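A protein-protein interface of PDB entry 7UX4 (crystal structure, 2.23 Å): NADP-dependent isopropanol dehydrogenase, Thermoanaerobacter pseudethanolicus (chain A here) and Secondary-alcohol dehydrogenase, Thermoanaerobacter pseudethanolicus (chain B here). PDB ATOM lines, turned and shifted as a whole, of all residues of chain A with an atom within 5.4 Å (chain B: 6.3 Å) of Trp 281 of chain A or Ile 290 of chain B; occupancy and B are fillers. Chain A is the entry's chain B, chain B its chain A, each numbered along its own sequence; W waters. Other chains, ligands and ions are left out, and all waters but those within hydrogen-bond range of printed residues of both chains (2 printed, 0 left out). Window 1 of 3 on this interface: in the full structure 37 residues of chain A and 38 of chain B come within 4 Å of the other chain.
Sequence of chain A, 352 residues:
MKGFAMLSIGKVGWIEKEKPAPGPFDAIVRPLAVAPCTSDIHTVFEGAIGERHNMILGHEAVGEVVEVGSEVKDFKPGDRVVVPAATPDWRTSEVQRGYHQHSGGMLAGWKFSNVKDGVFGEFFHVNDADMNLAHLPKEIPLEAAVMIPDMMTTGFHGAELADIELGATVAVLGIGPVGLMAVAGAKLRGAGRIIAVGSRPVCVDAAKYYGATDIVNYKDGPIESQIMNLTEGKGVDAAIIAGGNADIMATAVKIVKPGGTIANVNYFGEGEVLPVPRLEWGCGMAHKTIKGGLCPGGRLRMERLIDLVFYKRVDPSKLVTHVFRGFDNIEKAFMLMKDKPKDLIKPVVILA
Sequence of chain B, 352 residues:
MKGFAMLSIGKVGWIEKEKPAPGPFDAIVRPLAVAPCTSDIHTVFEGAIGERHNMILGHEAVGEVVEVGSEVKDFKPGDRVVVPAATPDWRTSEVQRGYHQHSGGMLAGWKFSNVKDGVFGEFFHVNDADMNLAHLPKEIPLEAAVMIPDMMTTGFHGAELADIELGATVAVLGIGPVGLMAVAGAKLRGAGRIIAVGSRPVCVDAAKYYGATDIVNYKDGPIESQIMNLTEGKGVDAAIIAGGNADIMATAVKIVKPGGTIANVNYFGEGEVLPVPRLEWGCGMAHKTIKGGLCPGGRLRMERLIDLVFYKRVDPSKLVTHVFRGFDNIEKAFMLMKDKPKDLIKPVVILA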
ATOM      1  N   VAL A 253       4.361   2.893  21.070  1.00  0.00           N
ATOM      2  CA  VAL A 253       5.305   1.933  21.637  1.00  0.00           C
ATOM      3  C   VAL A 253       4.651   0.564  21.783  1.00  0.00           C
ATOM      4  O   VAL A 253       5.288  -0.472  21.552  1.00  0.00           O
ATOM      5  CB  VAL A 253       5.841   2.448  22.987  1.00  0.00           C
ATOM      6  CG1 VAL A 253       6.703   1.392  23.661  1.00  0.00           C
ATOM      7  CG2 VAL A 253       6.622   3.742  22.798  1.00  0.00           C
ATOM      8  N   VAL A 276       6.148   7.233  27.932  1.00  0.00           N
ATOM      9  CA  VAL A 276       6.685   6.017  27.329  1.00  0.00           C
ATOM     10  C   VAL A 276       6.368   4.854  28.265  1.00  0.00           C
ATOM     11  O   VAL A 276       6.870   4.825  29.396  1.00  0.00           O
ATOM     12  CB  VAL A 276       8.195   6.118  27.068  1.00  0.00           C
ATOM     13  CG1 VAL A 276       8.739   4.772  26.627  1.00  0.00           C
ATOM     14  CG2 VAL A 276       8.472   7.168  26.003  1.00  0.00           C
ATOM     15  N   PRO A 277       5.546   3.889  27.850  1.00  0.00           N
ATOM     16  CA  PRO A 277       5.134   2.819  28.773  1.00  0.00           C
ATOM     17  C   PRO A 277       6.319   1.943  29.148  1.00  0.00           C
ATOM     18  O   PRO A 277       7.054   1.470  28.281  1.00  0.00           O
ATOM     19  CB  PRO A 277       4.087   2.034  27.971  1.00  0.00           C
ATOM     20  CG  PRO A 277       3.819   2.850  26.731  1.00  0.00           C
ATOM     21  CD  PRO A 277       5.044   3.666  26.487  1.00  0.00           C
ATOM     22  N   ARG A 278       6.502   1.732  30.452  1.00  0.00           N
ATOM     23  CA  ARG A 278       7.689   1.029  30.929  1.00  0.00           C
ATOM     24  C   ARG A 278       7.702  -0.425  30.460  1.00  0.00           C
ATOM     25  O   ARG A 278       8.694  -0.893  29.889  1.00  0.00           O
ATOM     26  CB  ARG A 278       7.768   1.105  32.452  1.00  0.00           C
ATOM     27  CG  ARG A 278       9.047   0.527  33.013  1.00  0.00           C
ATOM     28  CD  ARG A 278       9.079   0.620  34.523  1.00  0.00           C
ATOM     29  NE  ARG A 278       8.012  -0.178  35.113  1.00  0.00           N
ATOM     30  CZ  ARG A 278       8.120  -1.465  35.410  1.00  0.00           C
ATOM     31  NH1 ARG A 278       9.233  -2.138  35.169  1.00  0.00           N
ATOM     32  NH2 ARG A 278       7.079  -2.097  35.947  1.00  0.00           N
ATOM     33  N   LEU A 279       6.615  -1.161  30.712  1.00  0.00           N
ATOM     34  CA  LEU A 279       6.585  -2.584  30.377  1.00  0.00           C
ATOM     35  C   LEU A 279       6.658  -2.807  28.868  1.00  0.00           C
ATOM     36  O   LEU A 279       7.437  -3.644  28.394  1.00  0.00           O
ATOM     37  CB  LEU A 279       5.336  -3.241  30.969  1.00  0.00           C
ATOM     38  CG  LEU A 279       5.336  -3.400  32.494  1.00  0.00           C
ATOM     39  CD1 LEU A 279       4.078  -4.112  32.982  1.00  0.00           C
ATOM     40  CD2 LEU A 279       6.581  -4.143  32.949  1.00  0.00           C
ATOM     41  N   GLU A 280       5.858  -2.071  28.092  1.00  0.00           N
ATOM     42  CA  GLU A 280       5.866  -2.254  26.643  1.00  0.00           C
ATOM     43  C   GLU A 280       7.140  -1.742  25.981  1.00  0.00           C
ATOM     44  O   GLU A 280       7.365  -2.031  24.799  1.00  0.00           O
ATOM     45  CB  GLU A 280       4.650  -1.574  26.009  1.00  0.00           C
ATOM     46  CG  GLU A 280       3.332  -2.276  26.289  1.00  0.00           C
ATOM     47  CD  GLU A 280       2.739  -1.915  27.636  1.00  0.00           C
ATOM     48  OE1 GLU A 280       3.419  -1.219  28.422  1.00  0.00           O
ATOM     49  OE2 GLU A 280       1.592  -2.334  27.906  1.00  0.00           O
ATOM     50  N   TRP A 281       7.970  -0.985  26.694  1.00  0.00           N
ATOM     51  CA  TRP A 281       9.284  -0.609  26.202  1.00  0.00           C
ATOM     52  C   TRP A 281      10.365  -1.564  26.708  1.00  0.00           C
ATOM     53  O   TRP A 281      11.549  -1.214  26.709  1.00  0.00           O
ATOM     54  CB  TRP A 281       9.589   0.836  26.604  1.00  0.00           C
ATOM     55  CG  TRP A 281      10.526   1.564  25.694  1.00  0.00           C
ATOM     56  CD1 TRP A 281      10.397   1.726  24.344  1.00  0.00           C
ATOM     57  CD2 TRP A 281      11.720   2.260  26.068  1.00  0.00           C
ATOM     58  NE1 TRP A 281      11.444   2.468  23.853  1.00  0.00           N
ATOM     59  CE2 TRP A 281      12.272   2.807  24.891  1.00  0.00           C
ATOM     60  CE3 TRP A 281      12.381   2.468  27.281  1.00  0.00           C
ATOM     61  CZ2 TRP A 281      13.452   3.543  24.893  1.00  0.00           C
ATOM     62  CZ3 TRP A 281      13.554   3.201  27.281  1.00  0.00           C
ATOM     63  CH2 TRP A 281      14.076   3.730  26.096  1.00  0.00           C
ATOM     64  N   GLY A 282       9.973  -2.766  27.133  1.00  0.00           N
ATOM     65  CA  GLY A 282      10.930  -3.744  27.621  1.00  0.00           C
ATOM     66  C   GLY A 282      11.639  -3.325  28.886  1.00  0.00           C
ATOM     67  O   GLY A 282      12.759  -3.785  29.146  1.00  0.00           O
ATOM     68  N   CYS A 283      11.015  -2.455  29.684  1.00  0.00           N
ATOM     69  CA  CYS A 283      11.639  -1.878  30.874  1.00  0.00           C
ATOM     70  C   CYS A 283      12.949  -1.179  30.525  1.00  0.00           C
ATOM     71  O   CYS A 283      13.878  -1.126  31.337  1.00  0.00           O
ATOM     72  CB  CYS A 283      11.859  -2.940  31.953  1.00  0.00           C
ATOM     73  SG  CYS A 283      10.367  -3.869  32.385  1.00  0.00           S
ATOM     74  N   GLY A 284      13.024  -0.641  29.311  1.00  0.00           N
ATOM     75  CA  GLY A 284      14.207   0.033  28.826  1.00  0.00           C
ATOM     76  C   GLY A 284      15.086  -0.769  27.893  1.00  0.00           C
ATOM     77  O   GLY A 284      16.151  -0.277  27.506  1.00  0.00           O
ATOM     78  N   MET A 285      14.678  -1.983  27.509  1.00  0.00           N
ATOM     79  CA  MET A 285      15.595  -2.877  26.815  1.00  0.00           C
ATOM     80  C   MET A 285      14.946  -3.596  25.631  1.00  0.00           C
ATOM     81  O   MET A 285      15.421  -4.668  25.234  1.00  0.00           O
ATOM     82  CB  MET A 285      16.178  -3.899  27.811  1.00  0.00           C
ATOM     83  CG  MET A 285      16.989  -3.264  28.950  1.00  0.00           C
ATOM     84  SD  MET A 285      17.416  -4.377  30.307  1.00  0.00           S
ATOM     85  CE  MET A 285      15.801  -4.910  30.870  1.00  0.00           C
ATOM     86  N   ALA A 286      13.891  -3.033  25.046  1.00  0.00           N
ATOM     87  CA  ALA A 286      13.162  -3.689  23.968  1.00  0.00           C
ATOM     88  C   ALA A 286      13.649  -3.300  22.579  1.00  0.00           C
ATOM     89  O   ALA A 286      13.046  -3.731  21.590  1.00  0.00           O
ATOM     90  CB  ALA A 286      11.666  -3.380  24.080  1.00  0.00           C
ATOM     91  N   LYS A 288      13.210  -0.641  21.023  1.00  0.00           N
ATOM     92  CA  LYS A 288      12.189   0.129  20.316  1.00  0.00           C
ATOM     93  C   LYS A 288      12.678   1.566  20.221  1.00  0.00           C
ATOM     94  O   LYS A 288      12.550   2.344  21.168  1.00  0.00           O
ATOM     95  CB  LYS A 288      10.840   0.024  21.015  1.00  0.00           C
ATOM     96  CG  LYS A 288      10.313  -1.397  21.093  1.00  0.00           C
ATOM     97  CD  LYS A 288       8.872  -1.433  21.572  1.00  0.00           C
ATOM     98  CE  LYS A 288       8.405  -2.864  21.760  1.00  0.00           C
ATOM     99  NZ  LYS A 288       6.948  -2.948  22.062  1.00  0.00           N
ATOM    100  N   THR A 289      13.256   1.913  19.077  1.00  0.00           N
ATOM    101  CA  THR A 289      13.823   3.240  18.902  1.00  0.00           C
ATOM    102  C   THR A 289      12.722   4.277  18.730  1.00  0.00           C
ATOM    103  O   THR A 289      11.759   4.066  17.989  1.00  0.00           O
ATOM    104  CB  THR A 289      14.752   3.251  17.691  1.00  0.00           C
ATOM    105  OG1 THR A 289      15.749   2.233  17.851  1.00  0.00           O
ATOM    106  CG2 THR A 289      15.442   4.595  17.573  1.00  0.00           C
ATOM    107  N   ILE A 290      12.879   5.412  19.412  1.00  0.00           N
ATOM    108  CA  ILE A 290      11.925   6.518  19.359  1.00  0.00           C
ATOM    109  C   ILE A 290      12.640   7.721  18.763  1.00  0.00           C
ATOM    110  O   ILE A 290      13.618   8.213  19.340  1.00  0.00           O
ATOM    111  CB  ILE A 290      11.368   6.870  20.747  1.00  0.00           C
ATOM    112  CG1 ILE A 290      10.690   5.666  21.400  1.00  0.00           C
ATOM    113  CG2 ILE A 290      10.389   8.020  20.642  1.00  0.00           C
ATOM    114  CD1 ILE A 290      10.312   5.910  22.852  1.00  0.00           C
ATOM    115  N   LYS A 291      12.149   8.202  17.622  1.00  0.00           N
ATOM    116  CA  LYS A 291      12.694   9.378  16.963  1.00  0.00           C
ATOM    117  C   LYS A 291      11.631  10.464  16.861  1.00  0.00           C
ATOM    118  O   LYS A 291      10.431  10.181  16.800  1.00  0.00           O
ATOM    119  CB  LYS A 291      13.212   9.058  15.556  1.00  0.00           C
ATOM    120  CG  LYS A 291      14.287   7.991  15.484  1.00  0.00           C
ATOM    121  CD  LYS A 291      14.825   7.913  14.063  1.00  0.00           C
ATOM    122  CE  LYS A 291      15.765   6.741  13.864  1.00  0.00           C
ATOM    123  NZ  LYS A 291      16.121   6.586  12.423  1.00  0.00           N
ATOM    124  N   MET B 106       9.935 -10.614  23.534  1.00  0.00           N
ATOM    125  CA  MET B 106      10.696  -9.521  24.130  1.00  0.00           C
ATOM    126  C   MET B 106      11.579 -10.033  25.263  1.00  0.00           C
ATOM    127  O   MET B 106      11.088 -10.650  26.213  1.00  0.00           O
ATOM    128  CB  MET B 106       9.739  -8.443  24.634  1.00  0.00           C
ATOM    129  CG  MET B 106      10.394  -7.094  24.887  1.00  0.00           C
ATOM    130  SD  MET B 106       9.166  -5.827  25.259  1.00  0.00           S
ATOM    131  CE  MET B 106       8.273  -6.614  26.596  1.00  0.00           C
ATOM    132  N   MET B 249      15.427   9.544  32.760  1.00  0.00           N
ATOM    133  CA  MET B 249      15.146   9.685  31.336  1.00  0.00           C
ATOM    134  C   MET B 249      14.946  11.149  30.965  1.00  0.00           C
ATOM    135  O   MET B 249      15.435  11.608  29.924  1.00  0.00           O
ATOM    136  CB  MET B 249      13.908   8.861  30.970  1.00  0.00           C
ATOM    137  CG  MET B 249      13.414   9.037  29.535  1.00  0.00           C
ATOM    138  SD  MET B 249      14.590   8.515  28.275  1.00  0.00           S
ATOM    139  CE  MET B 249      14.692   6.755  28.600  1.00  0.00           C
ATOM    140  N   VAL B 253      17.303  13.553  28.333  1.00  0.00           N
ATOM    141  CA  VAL B 253      16.806  14.356  27.218  1.00  0.00           C
ATOM    142  C   VAL B 253      17.235  15.810  27.373  1.00  0.00           C
ATOM    143  O   VAL B 253      17.571  16.483  26.389  1.00  0.00           O
ATOM    144  CB  VAL B 253      15.275  14.228  27.122  1.00  0.00           C
ATOM    145  CG1 VAL B 253      14.715  15.191  26.088  1.00  0.00           C
ATOM    146  CG2 VAL B 253      14.884  12.794  26.789  1.00  0.00           C
ATOM    147  N   GLY B 260      21.286  14.822  19.058  1.00  0.00           N
ATOM    148  CA  GLY B 260      22.019  13.815  19.795  1.00  0.00           C
ATOM    149  C   GLY B 260      21.194  12.563  20.031  1.00  0.00           C
ATOM    150  O   GLY B 260      20.137  12.351  19.438  1.00  0.00           O
ATOM    151  N   THR B 261      21.698  11.718  20.933  1.00  0.00           N
ATOM    152  CA  THR B 261      21.110  10.407  21.176  1.00  0.00           C
ATOM    153  C   THR B 261      21.100  10.097  22.668  1.00  0.00           C
ATOM    154  O   THR B 261      22.076  10.368  23.374  1.00  0.00           O
ATOM    155  CB  THR B 261      21.884   9.309  20.427  1.00  0.00           C
ATOM    156  OG1 THR B 261      21.926   9.617  19.027  1.00  0.00           O
ATOM    157  CG2 THR B 261      21.220   7.949  20.621  1.00  0.00           C
ATOM    158  N   ILE B 262      19.989   9.536  23.143  1.00  0.00           N
ATOM    159  CA  ILE B 262      19.877   8.995  24.494  1.00  0.00           C
ATOM    160  C   ILE B 262      19.899   7.478  24.366  1.00  0.00           C
ATOM    161  O   ILE B 262      19.008   6.888  23.741  1.00  0.00           O
ATOM    162  CB  ILE B 262      18.599   9.470  25.207  1.00  0.00           C
ATOM    163  CG1 ILE B 262      18.631  10.978  25.465  1.00  0.00           C
ATOM    164  CG2 ILE B 262      18.415   8.732  26.521  1.00  0.00           C
ATOM    165  CD1 ILE B 262      17.998  11.800  24.359  1.00  0.00           C
ATOM    166  N   ALA B 263      20.922   6.847  24.931  1.00  0.00           N
ATOM    167  CA  ALA B 263      21.101   5.402  24.835  1.00  0.00           C
ATOM    168  C   ALA B 263      20.943   4.804  26.226  1.00  0.00           C
ATOM    169  O   ALA B 263      21.783   5.033  27.103  1.00  0.00           O
ATOM    170  CB  ALA B 263      22.465   5.063  24.242  1.00  0.00           C
ATOM    171  N   ASN B 264      19.881   4.028  26.424  1.00  0.00           N
ATOM    172  CA  ASN B 264      19.578   3.439  27.720  1.00  0.00           C
ATOM    173  C   ASN B 264      19.909   1.954  27.722  1.00  0.00           C
ATOM    174  O   ASN B 264      19.479   1.214  26.833  1.00  0.00           O
ATOM    175  CB  ASN B 264      18.106   3.627  28.087  1.00  0.00           C
ATOM    176  CG  ASN B 264      17.741   2.910  29.368  1.00  0.00           C
ATOM    177  OD1 ASN B 264      18.043   3.387  30.457  1.00  0.00           O
ATOM    178  ND2 ASN B 264      17.116   1.745  29.246  1.00  0.00           N
ATOM    179  N   PHE B 268      14.531  -0.277  34.210  1.00  0.00           N
ATOM    180  CA  PHE B 268      13.525   0.436  34.993  1.00  0.00           C
ATOM    181  C   PHE B 268      12.501  -0.571  35.502  1.00  0.00           C
ATOM    182  O   PHE B 268      11.722  -1.123  34.718  1.00  0.00           O
ATOM    183  CB  PHE B 268      12.864   1.529  34.154  1.00  0.00           C
ATOM    184  CG  PHE B 268      13.835   2.525  33.583  1.00  0.00           C
ATOM    185  CD1 PHE B 268      14.259   3.612  34.333  1.00  0.00           C
ATOM    186  CD2 PHE B 268      14.323   2.377  32.296  1.00  0.00           C
ATOM    187  CE1 PHE B 268      15.157   4.531  33.811  1.00  0.00           C
ATOM    188  CE2 PHE B 268      15.219   3.294  31.765  1.00  0.00           C
ATOM    189  CZ  PHE B 268      15.637   4.374  32.527  1.00  0.00           C
ATOM    190  N   LEU B 274       7.791   6.042  31.627  1.00  0.00           N
ATOM    191  CA  LEU B 274       9.070   6.741  31.668  1.00  0.00           C
ATOM    192  C   LEU B 274       8.885   8.128  31.079  1.00  0.00           C
ATOM    193  O   LEU B 274       8.432   8.244  29.931  1.00  0.00           O
ATOM    194  CB  LEU B 274      10.138   5.978  30.892  1.00  0.00           C
ATOM    195  CG  LEU B 274      10.370   4.512  31.268  1.00  0.00           C
ATOM    196  CD1 LEU B 274      11.577   3.969  30.519  1.00  0.00           C
ATOM    197  CD2 LEU B 274      10.542   4.345  32.774  1.00  0.00           C
ATOM    198  N   VAL B 276       9.321  11.543  29.171  1.00  0.00           N
ATOM    199  CA  VAL B 276      10.098  12.276  28.179  1.00  0.00           C
ATOM    200  C   VAL B 276       9.636  13.731  28.234  1.00  0.00           C
ATOM    201  O   VAL B 276       8.479  14.024  27.898  1.00  0.00           O
ATOM    202  CB  VAL B 276       9.931  11.690  26.772  1.00  0.00           C
ATOM    203  CG1 VAL B 276      10.618  12.583  25.750  1.00  0.00           C
ATOM    204  CG2 VAL B 276      10.494  10.277  26.721  1.00  0.00           C
ATOM    205  N   TRP B 281      12.371  18.012  24.618  1.00  0.00           N
ATOM    206  CA  TRP B 281      12.383  17.109  23.479  1.00  0.00           C
ATOM    207  C   TRP B 281      11.900  17.798  22.213  1.00  0.00           C
ATOM    208  O   TRP B 281      11.450  17.123  21.278  1.00  0.00           O
ATOM    209  CB  TRP B 281      11.532  15.870  23.773  1.00  0.00           C
ATOM    210  CG  TRP B 281      11.950  14.657  22.996  1.00  0.00           C
ATOM    211  CD1 TRP B 281      13.200  14.117  22.939  1.00  0.00           C
ATOM    212  CD2 TRP B 281      11.114  13.817  22.186  1.00  0.00           C
ATOM    213  NE1 TRP B 281      13.201  13.003  22.136  1.00  0.00           N
ATOM    214  CE2 TRP B 281      11.931  12.797  21.662  1.00  0.00           C
ATOM    215  CE3 TRP B 281       9.757  13.832  21.853  1.00  0.00           C
ATOM    216  CZ2 TRP B 281      11.437  11.800  20.819  1.00  0.00           C
ATOM    217  CZ3 TRP B 281       9.268  12.841  21.012  1.00  0.00           C
ATOM    218  CH2 TRP B 281      10.104  11.840  20.507  1.00  0.00           C
ATOM    219  N   LYS B 288      16.239  14.256  18.979  1.00  0.00           N
ATOM    220  CA  LYS B 288      16.926  13.582  20.082  1.00  0.00           C
ATOM    221  C   LYS B 288      16.458  12.131  20.086  1.00  0.00           C
ATOM    222  O   LYS B 288      15.394  11.812  20.620  1.00  0.00           O
ATOM    223  CB  LYS B 288      16.652  14.269  21.418  1.00  0.00           C
ATOM    224  CG  LYS B 288      17.111  15.727  21.499  1.00  0.00           C
ATOM    225  CD  LYS B 288      17.015  16.252  22.929  1.00  0.00           C
ATOM    226  CE  LYS B 288      17.339  17.730  22.998  1.00  0.00           C
ATOM    227  NZ  LYS B 288      17.410  18.212  24.404  1.00  0.00           N
ATOM    228  N   THR B 289      17.256  11.254  19.483  1.00  0.00           N
ATOM    229  CA  THR B 289      16.884   9.849  19.367  1.00  0.00           C
ATOM    230  C   THR B 289      17.012   9.143  20.711  1.00  0.00           C
ATOM    231  O   THR B 289      17.975   9.358  21.454  1.00  0.00           O
ATOM    232  CB  THR B 289      17.763   9.164  18.327  1.00  0.00           C
ATOM    233  OG1 THR B 289      17.648   9.862  17.081  1.00  0.00           O
ATOM    234  CG2 THR B 289      17.334   7.719  18.130  1.00  0.00           C
ATOM    235  N   ILE B 290      16.029   8.307  21.035  1.00  0.00           N
ATOM    236  CA  ILE B 290      16.019   7.555  22.287  1.00  0.00           C
ATOM    237  C   ILE B 290      16.054   6.069  21.957  1.00  0.00           C
ATOM    238  O   ILE B 290      15.131   5.548  21.318  1.00  0.00           O
ATOM    239  CB  ILE B 290      14.790   7.887  23.144  1.00  0.00           C
ATOM    240  CG1 ILE B 290      14.735   9.382  23.443  1.00  0.00           C
ATOM    241  CG2 ILE B 290      14.826   7.095  24.443  1.00  0.00           C
ATOM    242  CD1 ILE B 290      13.444   9.808  24.094  1.00  0.00           C
ATOM    243  N   LYS B 291      17.104   5.390  22.409  1.00  0.00           N
ATOM    244  CA  LYS B 291      17.263   3.956  22.226  1.00  0.00           C
ATOM    245  C   LYS B 291      17.339   3.269  23.582  1.00  0.00           C
ATOM    246  O   LYS B 291      17.793   3.855  24.569  1.00  0.00           O
ATOM    247  CB  LYS B 291      18.534   3.635  21.445  1.00  0.00           C
ATOM    248  CG  LYS B 291      18.654   4.287  20.089  1.00  0.00           C
ATOM    249  CD  LYS B 291      19.899   3.754  19.414  1.00  0.00           C
ATOM    250  CE  LYS B 291      20.242   4.504  18.148  1.00  0.00           C
ATOM    251  NZ  LYS B 291      21.579   4.071  17.645  1.00  0.00           N
ATOM    252  N   GLY B 292      16.917   2.009  23.618  1.00  0.00           N
ATOM    253  CA  GLY B 292      17.025   1.219  24.829  1.00  0.00           C
ATOM    254  C   GLY B 292      17.032  -0.263  24.521  1.00  0.00           C
ATOM    255  O   GLY B 292      16.018  -0.797  24.066  1.00  0.00           O
HETATM  256  O   HOH W   1      16.758   1.030  20.569  1.00  0.00           O
HETATM  257  O   HOH W   2      13.255  -0.404  24.009  1.00  0.00           O
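Printed residues of chain B within 4 Å of Arg 278 of chain A: Phe 268 (2.7 Å).
Of the printed residues of chain B, Trp 281 of chain A touches Met 249, Leu 274, Ile 290 and Gly 292.
Thr 261 of chain B touches none of the printed residues of chain A.
Printed residues of chain A within 4 Å of Thr 289 of chain B: Thr 289 and Ile 290.
Of the printed residues of chain A, Ile 290 of chain B touches Trp 281, Thr 289 and Ile 290.
The nearest printed residue of chain B that does not touch Trp 281 of chain A is Lys 291 of chain B (4.02 Å).
The nearest printed residue of chain B that does not touch Cys 283 of chain A is Asn 264 of chain B (4.8 Å).
O of Gly 260 of chain B sits at hydrogen-bond distance from N of Thr 289 of chain B (3.1 Å).
The backbone NH (N) of Ile 262 of chain B sits at hydrogen-bond distance from the backbone carbonyl oxygen (O) of Thr 289 of chain B (2.6 Å).
N of Asn 264 of chain B lies within hydrogen-bond range of O of Lys 291 of chain B (2.8 Å).
The backbone NH of Cys 283 of chain A lies within hydrogen-bond range of the backbone carbonyl oxygen of Arg 278 of chain A, 2.8 Å away.
The backbone carbonyl oxygen (O) of Trp 281 of chain A is in hydrogen-bond range of the backbone NH (N) of Ala 286 of chain A, at 3.4 Å.
The indole nitrogen (NE1) of Trp 281 of chain A is in hydrogen-bond range of the backbone carbonyl oxygen (O) of Lys 288 of chain A.
Among the printed residues, pairs that only touch across the chains: Val 276 of chain A with Val 276 of chain B (3.8 Å), Leu 279 of chain A with Met 106 of chain B (3.6 Å), Trp 281 of chain A with Met 249 of chain B (3.96 Å), Trp 281 of chain A with Leu 274 of chain B (3.7 Å), Trp 281 of chain A with Ile 290 of chain B (3.8 Å), Trp 281 of chain A with Gly 292 of chain B (3.998 Å), Met 285 of chain A with Gly 292 of chain B (3.4 Å), Ala 286 of chain A with Met 106 of chain B (3.7 Å), Thr 289 of chain A with Thr 289 of chain B (3.7 Å), Thr 289 of chain A with Ile 290 of chain B (3.6 Å), Ile 290 of chain A with Trp 281 of chain B (3.8 Å) and Ile 290 of chain A with Thr 289 of chain B (3.7 Å).
Water W2 lies within hydrogen-bond range of O of Gly 292 of chain B (2.8 Å), N of Ala 286 of chain A (2.9 Å), N of Lys 288 of chain A (3.0 Å) and O of Trp 281 of chain A (3.3 Å).
Water W1 bridges OG1 of Thr 289 of chain A (3.1 Å) and N of Gly 292 of chain B (3.2 Å).
Of the 17 printed residues of chain B, 10 touch a printed residue of chain A.
Hydrophobic or aromatic side chains of chain B within 4 Å of the printed part of chain A: Met 106, Met 249, Phe 268, Leu 274, Val 276, Trp 281 and Ile 290.
Printed residues of chain A that touch a printed residue of chain B: Val 276, Arg 278, Leu 279, Trp 281, Gly 282, Cys 283, Gly 284, Met 285, Ala 286, Thr 289 and Ile 290.
Among the printed residues, 20 pairs touch across the chains.
Among the printed residues, no Asp or Glu carboxylate lies within 4 Å of a Lys or Arg side-chain nitrogen of the other chain.
SD of Met 106 of chain B lies close to N of Gly 282 of chain A (3.7 Å).
The backbone carbonyl oxygen (O) of Gly 284 of chain A lies within hydrogen-bond range of the side-chain amide nitrogen (ND2) of Asn 264 of chain B (2.8 Å).
The guanidinium group of Arg 278 of chain A is in hydrogen-bond range of the backbone carbonyl oxygen of Phe 268 of chain B.
The backbone carbonyl oxygen (O) of Cys 283 of chain A is in hydrogen-bond range of the backbone NH (N) of Phe 268 of chain B, at 3.1 Å.
The backbone carbonyl oxygen (O) of Val 276 of chain A lies within hydrogen-bond range of the backbone NH (N) of Leu 274 of chain B, 2.7 Å away.
The backbone carbonyl oxygen of Ile 290 of chain A sits at hydrogen-bond distance from the backbone NH of Ile 290 of chain B (2.9 Å).
N of Ala 286 of chain A is in hydrogen-bond range of O of Gly 292 of chain B.
The backbone carbonyl oxygen (O) of Gly 284 of chain A sits close to the backbone carbonyl oxygen (O) of Gly 292 of chain B.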
